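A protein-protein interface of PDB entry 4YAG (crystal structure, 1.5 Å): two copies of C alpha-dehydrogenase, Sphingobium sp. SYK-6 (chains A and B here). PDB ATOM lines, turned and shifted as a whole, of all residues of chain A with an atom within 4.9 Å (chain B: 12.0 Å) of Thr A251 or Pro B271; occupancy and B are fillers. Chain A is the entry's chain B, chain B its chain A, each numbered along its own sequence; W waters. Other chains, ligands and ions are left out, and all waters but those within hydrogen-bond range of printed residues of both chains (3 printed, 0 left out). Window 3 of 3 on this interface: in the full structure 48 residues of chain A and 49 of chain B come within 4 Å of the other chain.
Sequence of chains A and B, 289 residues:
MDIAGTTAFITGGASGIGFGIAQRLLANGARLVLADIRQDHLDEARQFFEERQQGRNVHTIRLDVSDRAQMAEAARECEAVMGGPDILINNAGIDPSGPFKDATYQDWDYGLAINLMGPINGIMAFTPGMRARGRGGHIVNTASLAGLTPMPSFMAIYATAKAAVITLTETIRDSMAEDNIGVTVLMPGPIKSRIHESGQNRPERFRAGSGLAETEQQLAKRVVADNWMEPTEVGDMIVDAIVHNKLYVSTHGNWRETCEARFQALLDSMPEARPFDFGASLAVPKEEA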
ATOM      1  N   LEU A 186      13.372 -16.797   1.114  1.00  0.00           N
ATOM      2  CA  LEU A 186      13.499 -18.175   0.661  1.00  0.00           C
ATOM      3  C   LEU A 186      12.850 -18.273  -0.712  1.00  0.00           C
ATOM      4  O   LEU A 186      11.698 -17.887  -0.869  1.00  0.00           O
ATOM      5  CB  LEU A 186      12.767 -19.069   1.656  1.00  0.00           C
ATOM      6  CG  LEU A 186      12.537 -20.531   1.242  1.00  0.00           C
ATOM      7  CD1 LEU A 186      13.858 -21.265   1.059  1.00  0.00           C
ATOM      8  CD2 LEU A 186      11.671 -21.199   2.286  1.00  0.00           C
ATOM      9  N   MET A 187      13.603 -18.769  -1.692  1.00  0.00           N
ATOM     10  CA  MET A 187      13.139 -18.919  -3.070  1.00  0.00           C
ATOM     11  C   MET A 187      13.200 -20.386  -3.474  1.00  0.00           C
ATOM     12  O   MET A 187      14.230 -20.869  -3.949  1.00  0.00           O
ATOM     13  CB  MET A 187      14.016 -18.072  -3.989  1.00  0.00           C
ATOM     14  CG  MET A 187      13.861 -16.575  -3.717  1.00  0.00           C
ATOM     15  SD  MET A 187      15.149 -15.481  -4.408  1.00  0.00           S
ATOM     16  CE  MET A 187      16.556 -15.975  -3.416  1.00  0.00           C
ATOM     17  N   PRO A 188      12.098 -21.104  -3.251  1.00  0.00           N
ATOM     18  CA  PRO A 188      12.174 -22.529  -3.569  1.00  0.00           C
ATOM     19  C   PRO A 188      11.954 -22.858  -5.042  1.00  0.00           C
ATOM     20  O   PRO A 188      11.252 -22.115  -5.771  1.00  0.00           O
ATOM     21  CB  PRO A 188      11.035 -23.136  -2.736  1.00  0.00           C
ATOM     22  CG  PRO A 188      10.683 -22.102  -1.723  1.00  0.00           C
ATOM     23  CD  PRO A 188      10.930 -20.800  -2.411  1.00  0.00           C
ATOM     24  N   GLY A 189      12.564 -23.976  -5.451  1.00  0.00           N
ATOM     25  CA  GLY A 189      12.118 -24.752  -6.597  1.00  0.00           C
ATOM     26  C   GLY A 189      11.097 -25.761  -6.103  1.00  0.00           C
ATOM     27  O   GLY A 189      10.428 -25.518  -5.092  1.00  0.00           O
ATOM     28  N   ILE A 191       9.197 -28.335  -4.219  1.00  0.00           N
ATOM     29  CA  ILE A 191       9.212 -28.968  -2.915  1.00  0.00           C
ATOM     30  C   ILE A 191       7.934 -29.798  -2.733  1.00  0.00           C
ATOM     31  O   ILE A 191       6.838 -29.351  -3.062  1.00  0.00           O
ATOM     32  CB  ILE A 191       9.252 -27.926  -1.771  1.00  0.00           C
ATOM     33  CG1 ILE A 191      10.248 -26.799  -2.069  1.00  0.00           C
ATOM     34  CG2 ILE A 191       9.557 -28.647  -0.438  1.00  0.00           C
ATOM     35  CD1 ILE A 191      11.687 -27.277  -2.291  1.00  0.00           C
ATOM     36  N   MET A 229      11.971 -31.909  -3.658  1.00  0.00           N
ATOM     37  CA  MET A 229      12.713 -31.842  -2.416  1.00  0.00           C
ATOM     38  C   MET A 229      11.803 -32.051  -1.203  1.00  0.00           C
ATOM     39  O   MET A 229      10.625 -31.677  -1.217  1.00  0.00           O
ATOM     40  CB  MET A 229      13.398 -30.478  -2.320  1.00  0.00           C
ATOM     41  CG  MET A 229      14.266 -30.283  -1.097  1.00  0.00           C
ATOM     42  SD  MET A 229      15.253 -28.778  -1.210  1.00  0.00           S
ATOM     43  CE  MET A 229      16.437 -29.206  -2.469  1.00  0.00           C
ATOM     44  N   VAL A 234      14.564 -28.195   3.246  1.00  0.00           N
ATOM     45  CA  VAL A 234      14.388 -26.738   3.207  1.00  0.00           C
ATOM     46  C   VAL A 234      14.466 -26.161   4.629  1.00  0.00           C
ATOM     47  O   VAL A 234      15.067 -25.114   4.865  1.00  0.00           O
ATOM     48  CB  VAL A 234      13.045 -26.355   2.559  1.00  0.00           C
ATOM     49  CG1 VAL A 234      12.880 -24.820   2.505  1.00  0.00           C
ATOM     50  CG2 VAL A 234      12.914 -26.949   1.174  1.00  0.00           C
ATOM     51  N   MET A 237      17.928 -25.548   5.576  1.00  0.00           N
ATOM     52  CA  MET A 237      18.471 -24.376   4.890  1.00  0.00           C
ATOM     53  C   MET A 237      18.048 -23.106   5.620  1.00  0.00           C
ATOM     54  O   MET A 237      18.802 -22.134   5.688  1.00  0.00           O
ATOM     55  CB  MET A 237      17.995 -24.312   3.428  1.00  0.00           C
ATOM     56  CG  MET A 237      18.513 -25.432   2.555  1.00  0.00           C
ATOM     57  SD  MET A 237      17.800 -25.262   0.903  1.00  0.00           S
ATOM     58  CE  MET A 237      18.356 -26.770   0.147  1.00  0.00           C
ATOM     59  N   VAL A 249      18.122 -17.438   0.220  1.00  0.00           N
ATOM     60  CA  VAL A 249      18.207 -18.889   0.208  1.00  0.00           C
ATOM     61  C   VAL A 249      17.455 -19.403  -1.008  1.00  0.00           C
ATOM     62  O   VAL A 249      16.284 -19.111  -1.170  1.00  0.00           O
ATOM     63  CB  VAL A 249      17.615 -19.525   1.477  1.00  0.00           C
ATOM     64  CG1 VAL A 249      17.604 -21.054   1.360  1.00  0.00           C
ATOM     65  CG2 VAL A 249      18.433 -19.129   2.696  1.00  0.00           C
ATOM     66  N   SER A 250      18.169 -20.108  -1.887  1.00  0.00           N
ATOM     67  CA  SER A 250      17.551 -20.770  -3.022  1.00  0.00           C
ATOM     68  C   SER A 250      17.719 -22.273  -2.845  1.00  0.00           C
ATOM     69  O   SER A 250      18.808 -22.735  -2.485  1.00  0.00           O
ATOM     70  CB  SER A 250      18.212 -20.342  -4.327  1.00  0.00           C
ATOM     71  OG  SER A 250      17.968 -18.969  -4.587  1.00  0.00           O
ATOM     72  N   THR A 251      16.666 -23.039  -3.106  1.00  0.00           N
ATOM     73  CA  THR A 251      16.715 -24.475  -2.839  1.00  0.00           C
ATOM     74  C   THR A 251      17.228 -25.301  -4.010  1.00  0.00           C
ATOM     75  O   THR A 251      17.660 -26.432  -3.818  1.00  0.00           O
ATOM     76  CB  THR A 251      15.329 -25.064  -2.452  1.00  0.00           C
ATOM     77  OG1 THR A 251      14.435 -24.929  -3.559  1.00  0.00           O
ATOM     78  CG2 THR A 251      14.751 -24.387  -1.231  1.00  0.00           C
ATOM     79  N   HIS A 252      17.170 -24.736  -5.208  1.00  0.00           N
ATOM     80  CA  HIS A 252      17.534 -25.436  -6.430  1.00  0.00           C
ATOM     81  C   HIS A 252      18.366 -24.556  -7.317  1.00  0.00           C
ATOM     82  O   HIS A 252      18.199 -23.337  -7.308  1.00  0.00           O
ATOM     83  CB  HIS A 252      16.290 -25.816  -7.224  1.00  0.00           C
ATOM     84  CG  HIS A 252      15.505 -26.938  -6.630  1.00  0.00           C
ATOM     85  ND1 HIS A 252      14.757 -26.797  -5.481  1.00  0.00           N
ATOM     86  CD2 HIS A 252      15.350 -28.225  -7.025  1.00  0.00           C
ATOM     87  CE1 HIS A 252      14.174 -27.948  -5.197  1.00  0.00           C
ATOM     88  NE2 HIS A 252      14.512 -28.831  -6.125  1.00  0.00           N
ATOM     89  N   GLY A 253      19.201 -25.185  -8.138  1.00  0.00           N
ATOM     90  CA  GLY A 253      20.063 -24.483  -9.077  1.00  0.00           C
ATOM     91  C   GLY A 253      19.634 -24.584 -10.537  1.00  0.00           C
ATOM     92  O   GLY A 253      20.313 -24.068 -11.433  1.00  0.00           O
ATOM     93  N   ARG A 256      19.480 -21.348 -12.744  1.00  0.00           N
ATOM     94  CA  ARG A 256      20.633 -20.455 -12.825  1.00  0.00           C
ATOM     95  C   ARG A 256      20.769 -19.847 -14.233  1.00  0.00           C
ATOM     96  O   ARG A 256      20.848 -18.619 -14.387  1.00  0.00           O
ATOM     97  CB  ARG A 256      21.912 -21.182 -12.390  1.00  0.00           C
ATOM     98  CG  ARG A 256      23.196 -20.422 -12.683  1.00  0.00           C
ATOM     99  CD  ARG A 256      24.411 -21.274 -12.304  1.00  0.00           C
ATOM    100  NE  ARG A 256      24.355 -21.639 -10.894  1.00  0.00           N
ATOM    101  CZ  ARG A 256      24.829 -20.876  -9.910  1.00  0.00           C
ATOM    102  NH1 ARG A 256      25.432 -19.726 -10.181  1.00  0.00           N
ATOM    103  NH2 ARG A 256      24.722 -21.271  -8.654  1.00  0.00           N
ATOM    104  N   PHE B 263      22.444  -9.333  -8.786  1.00  0.00           N
ATOM    105  CA  PHE B 263      22.259 -10.530  -9.602  1.00  0.00           C
ATOM    106  C   PHE B 263      23.269 -11.615  -9.213  1.00  0.00           C
ATOM    107  O   PHE B 263      22.930 -12.787  -9.087  1.00  0.00           O
ATOM    108  CB  PHE B 263      22.415 -10.185 -11.082  1.00  0.00           C
ATOM    109  CG  PHE B 263      21.384  -9.221 -11.604  1.00  0.00           C
ATOM    110  CD1 PHE B 263      20.163  -9.042 -10.955  1.00  0.00           C
ATOM    111  CD2 PHE B 263      21.610  -8.521 -12.780  1.00  0.00           C
ATOM    112  CE1 PHE B 263      19.230  -8.148 -11.448  1.00  0.00           C
ATOM    113  CE2 PHE B 263      20.675  -7.649 -13.280  1.00  0.00           C
ATOM    114  CZ  PHE B 263      19.492  -7.461 -12.623  1.00  0.00           C
ATOM    115  N   GLN B 264      24.526 -11.237  -9.023  1.00  0.00           N
ATOM    116  CA  GLN B 264      25.507 -12.216  -8.567  1.00  0.00           C
ATOM    117  C   GLN B 264      25.176 -12.816  -7.216  1.00  0.00           C
ATOM    118  O   GLN B 264      25.369 -14.009  -7.011  1.00  0.00           O
ATOM    119  CB  GLN B 264      26.894 -11.597  -8.553  1.00  0.00           C
ATOM    120  CG  GLN B 264      27.408 -11.413  -9.952  1.00  0.00           C
ATOM    121  CD  GLN B 264      27.547 -12.753 -10.667  1.00  0.00           C
ATOM    122  OE1 GLN B 264      28.051 -13.712 -10.096  1.00  0.00           O
ATOM    123  NE2 GLN B 264      27.056 -12.828 -11.906  1.00  0.00           N
ATOM    124  N   ALA B 265      24.692 -12.007  -6.279  1.00  0.00           N
ATOM    125  CA  ALA B 265      24.319 -12.518  -4.974  1.00  0.00           C
ATOM    126  C   ALA B 265      23.145 -13.501  -5.087  1.00  0.00           C
ATOM    127  O   ALA B 265      23.131 -14.546  -4.429  1.00  0.00           O
ATOM    128  CB  ALA B 265      24.007 -11.389  -4.000  1.00  0.00           C
ATOM    129  N   LEU B 266      22.189 -13.189  -5.955  1.00  0.00           N
ATOM    130  CA  LEU B 266      21.084 -14.110  -6.214  1.00  0.00           C
ATOM    131  C   LEU B 266      21.597 -15.423  -6.812  1.00  0.00           C
ATOM    132  O   LEU B 266      21.238 -16.507  -6.367  1.00  0.00           O
ATOM    133  CB  LEU B 266      20.044 -13.445  -7.131  1.00  0.00           C
ATOM    134  CG  LEU B 266      19.242 -12.297  -6.499  1.00  0.00           C
ATOM    135  CD1 LEU B 266      18.586 -11.437  -7.549  1.00  0.00           C
ATOM    136  CD2 LEU B 266      18.208 -12.845  -5.530  1.00  0.00           C
ATOM    137  N   LEU B 267      22.440 -15.334  -7.830  1.00  0.00           N
ATOM    138  CA  LEU B 267      22.987 -16.553  -8.433  1.00  0.00           C
ATOM    139  C   LEU B 267      23.818 -17.337  -7.430  1.00  0.00           C
ATOM    140  O   LEU B 267      23.743 -18.575  -7.382  1.00  0.00           O
ATOM    141  CB  LEU B 267      23.808 -16.198  -9.673  1.00  0.00           C
ATOM    142  CG  LEU B 267      22.990 -15.534 -10.786  1.00  0.00           C
ATOM    143  CD1 LEU B 267      23.904 -15.005 -11.873  1.00  0.00           C
ATOM    144  CD2 LEU B 267      21.977 -16.506 -11.379  1.00  0.00           C
ATOM    145  N   ASP B 268      24.619 -16.640  -6.630  1.00  0.00           N
ATOM    146  CA  ASP B 268      25.447 -17.315  -5.624  1.00  0.00           C
ATOM    147  C   ASP B 268      24.644 -18.124  -4.606  1.00  0.00           C
ATOM    148  O   ASP B 268      25.184 -19.063  -4.006  1.00  0.00           O
ATOM    149  CB  ASP B 268      26.308 -16.322  -4.849  1.00  0.00           C
ATOM    150  CG  ASP B 268      27.453 -15.772  -5.667  1.00  0.00           C
ATOM    151  OD1 ASP B 268      27.690 -16.256  -6.797  1.00  0.00           O
ATOM    152  OD2 ASP B 268      28.116 -14.842  -5.163  1.00  0.00           O
ATOM    153  N   SER B 269      23.388 -17.753  -4.375  1.00  0.00           N
ATOM    154  CA  SER B 269      22.545 -18.463  -3.417  1.00  0.00           C
ATOM    155  C   SER B 269      22.055 -19.802  -3.986  1.00  0.00           C
ATOM    156  O   SER B 269      21.490 -20.612  -3.256  1.00  0.00           O
ATOM    157  CB  SER B 269      21.329 -17.642  -2.970  1.00  0.00           C
ATOM    158  OG  SER B 269      20.322 -17.527  -3.979  1.00  0.00           O
ATOM    159  N   MET B 270      22.233 -20.010  -5.284  1.00  0.00           N
ATOM    160  CA  MET B 270      21.710 -21.216  -5.921  1.00  0.00           C
ATOM    161  C   MET B 270      22.731 -22.340  -5.883  1.00  0.00           C
ATOM    162  O   MET B 270      23.889 -22.137  -6.233  1.00  0.00           O
ATOM    163  CB  MET B 270      21.338 -20.945  -7.363  1.00  0.00           C
ATOM    164  CG  MET B 270      20.299 -19.831  -7.493  1.00  0.00           C
ATOM    165  SD  MET B 270      19.934 -19.446  -9.222  1.00  0.00           S
ATOM    166  CE  MET B 270      18.804 -18.090  -9.039  1.00  0.00           C
ATOM    167  N   PRO B 271      22.297 -23.533  -5.480  1.00  0.00           N
ATOM    168  CA  PRO B 271      23.209 -24.686  -5.485  1.00  0.00           C
ATOM    169  C   PRO B 271      23.361 -25.298  -6.866  1.00  0.00           C
ATOM    170  O   PRO B 271      23.020 -24.648  -7.849  1.00  0.00           O
ATOM    171  CB  PRO B 271      22.511 -25.675  -4.561  1.00  0.00           C
ATOM    172  CG  PRO B 271      21.073 -25.372  -4.719  1.00  0.00           C
ATOM    173  CD  PRO B 271      20.972 -23.882  -4.948  1.00  0.00           C
HETATM  174  O   HOH W   1      27.151 -18.036  -8.626  1.00  0.00           O
HETATM  175  O   HOH W   2      20.898 -20.838  -0.710  1.00  0.00           O
HETATM  176  O   HOH W   3      17.869 -21.955  -9.725  1.00  0.00           O
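Met B270 touches Ser A250. Ser A250 touches Pro B271. CG of Pro B271 touches O of Thr A251 (3.7 Å). Met B270 touches His A252 (CB to O, 3.9 Å). Pro B271 touches His A252 (CD to C, 3.6 Å). Pro B271 touches Gly A253. Arg A256 touches Pro B271.
The backbone carbonyl oxygen of Met B270 sits at hydrogen-bond distance from the guanidinium group of Arg A256. The backbone carbonyl oxygen (O) of Leu B267 lies within hydrogen-bond range of the guanidinium group (NH2) of Arg A256, at 3.1 Å. The side-chain hydroxyl of Ser B269 lies within hydrogen-bond range of the side-chain hydroxyl of Ser A250 (2.8 Å).
O of Met A187 lies within hydrogen-bond range of N of Thr A251, at 3.4 Å. The side-chain hydroxyl (OG) of Ser B269 lies within hydrogen-bond range of the backbone carbonyl oxygen (O) of Leu B266 (2.8 Å). N of Gly A189 sits at hydrogen-bond distance from OG1 of Thr A251 (2.8 Å). OG1 of Thr A251 lies within hydrogen-bond range of ND1 of His A252.
Water W1 lies within hydrogen-bond range of OD1 of Asp B268 (2.6 Å) and NH1 of Arg A256 (2.9 Å). Water W2 lies within hydrogen-bond range of O of Ser B269 and N of Ser A250. Water W3 lies within hydrogen-bond range of O of His A252 (2.8 Å), SD of Met B270 (3.3 Å) and N of Arg A256 (3.5 Å).
No position is printed for both chains. Of the 10 pairs that touch across the chains among the printed residues, none has its exchanged pair printed and touching as well.
Of the 14 printed residues of chain A, 5 touch a printed residue of chain B. Printed residues of chain B that touch a printed residue of chain A: Leu B267, Ser B269, Met B270 and Pro B271. Hydrophobic or aromatic side chains of chain B that line the printed part of chain A: Leu B267, Met B270 and Pro B271. Among the printed residues, 10 pairs touch across the chains.
Met A187 touches none of the printed residues of chain B. No residue of chain B comes within 4 Å of Pro A188. No residue of chain B comes within 4 Å of Gly A189. Ile A191 touches none of the printed residues of chain B. Met A229 touches none of the printed residues of chain B. Ser A250 touches three residues of chain B. Thr A251 touches just one residue of chain B: Pro B271 (3.7 Å). Gly A253 touches one residue of chain B. Printed residues of chain B within 4 Å of Arg A256: Leu B267, Met B270 and Pro B271. Of the printed residues of chain A, Leu B267 touches Arg A256 (3.1 Å). Of the printed residues of chain A, Ser B269 touches Ser A250 (2.8 Å). Of the printed residues of chain A, Met B270 touches Ser A250 (3.8 Å), His A252 (3.9 Å) and Arg A256 (2.7 Å). Pro B271 touches just these residues of chain A: Ser A250 (3.5 Å), Thr A251 (3.7 Å), His A252 (3.6 Å), Gly A253 (3.2 Å) and Arg A256 (3.9 Å). The nearest residue of chain B that does not touch Thr A251 is Ser B269 (5.4 Å).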
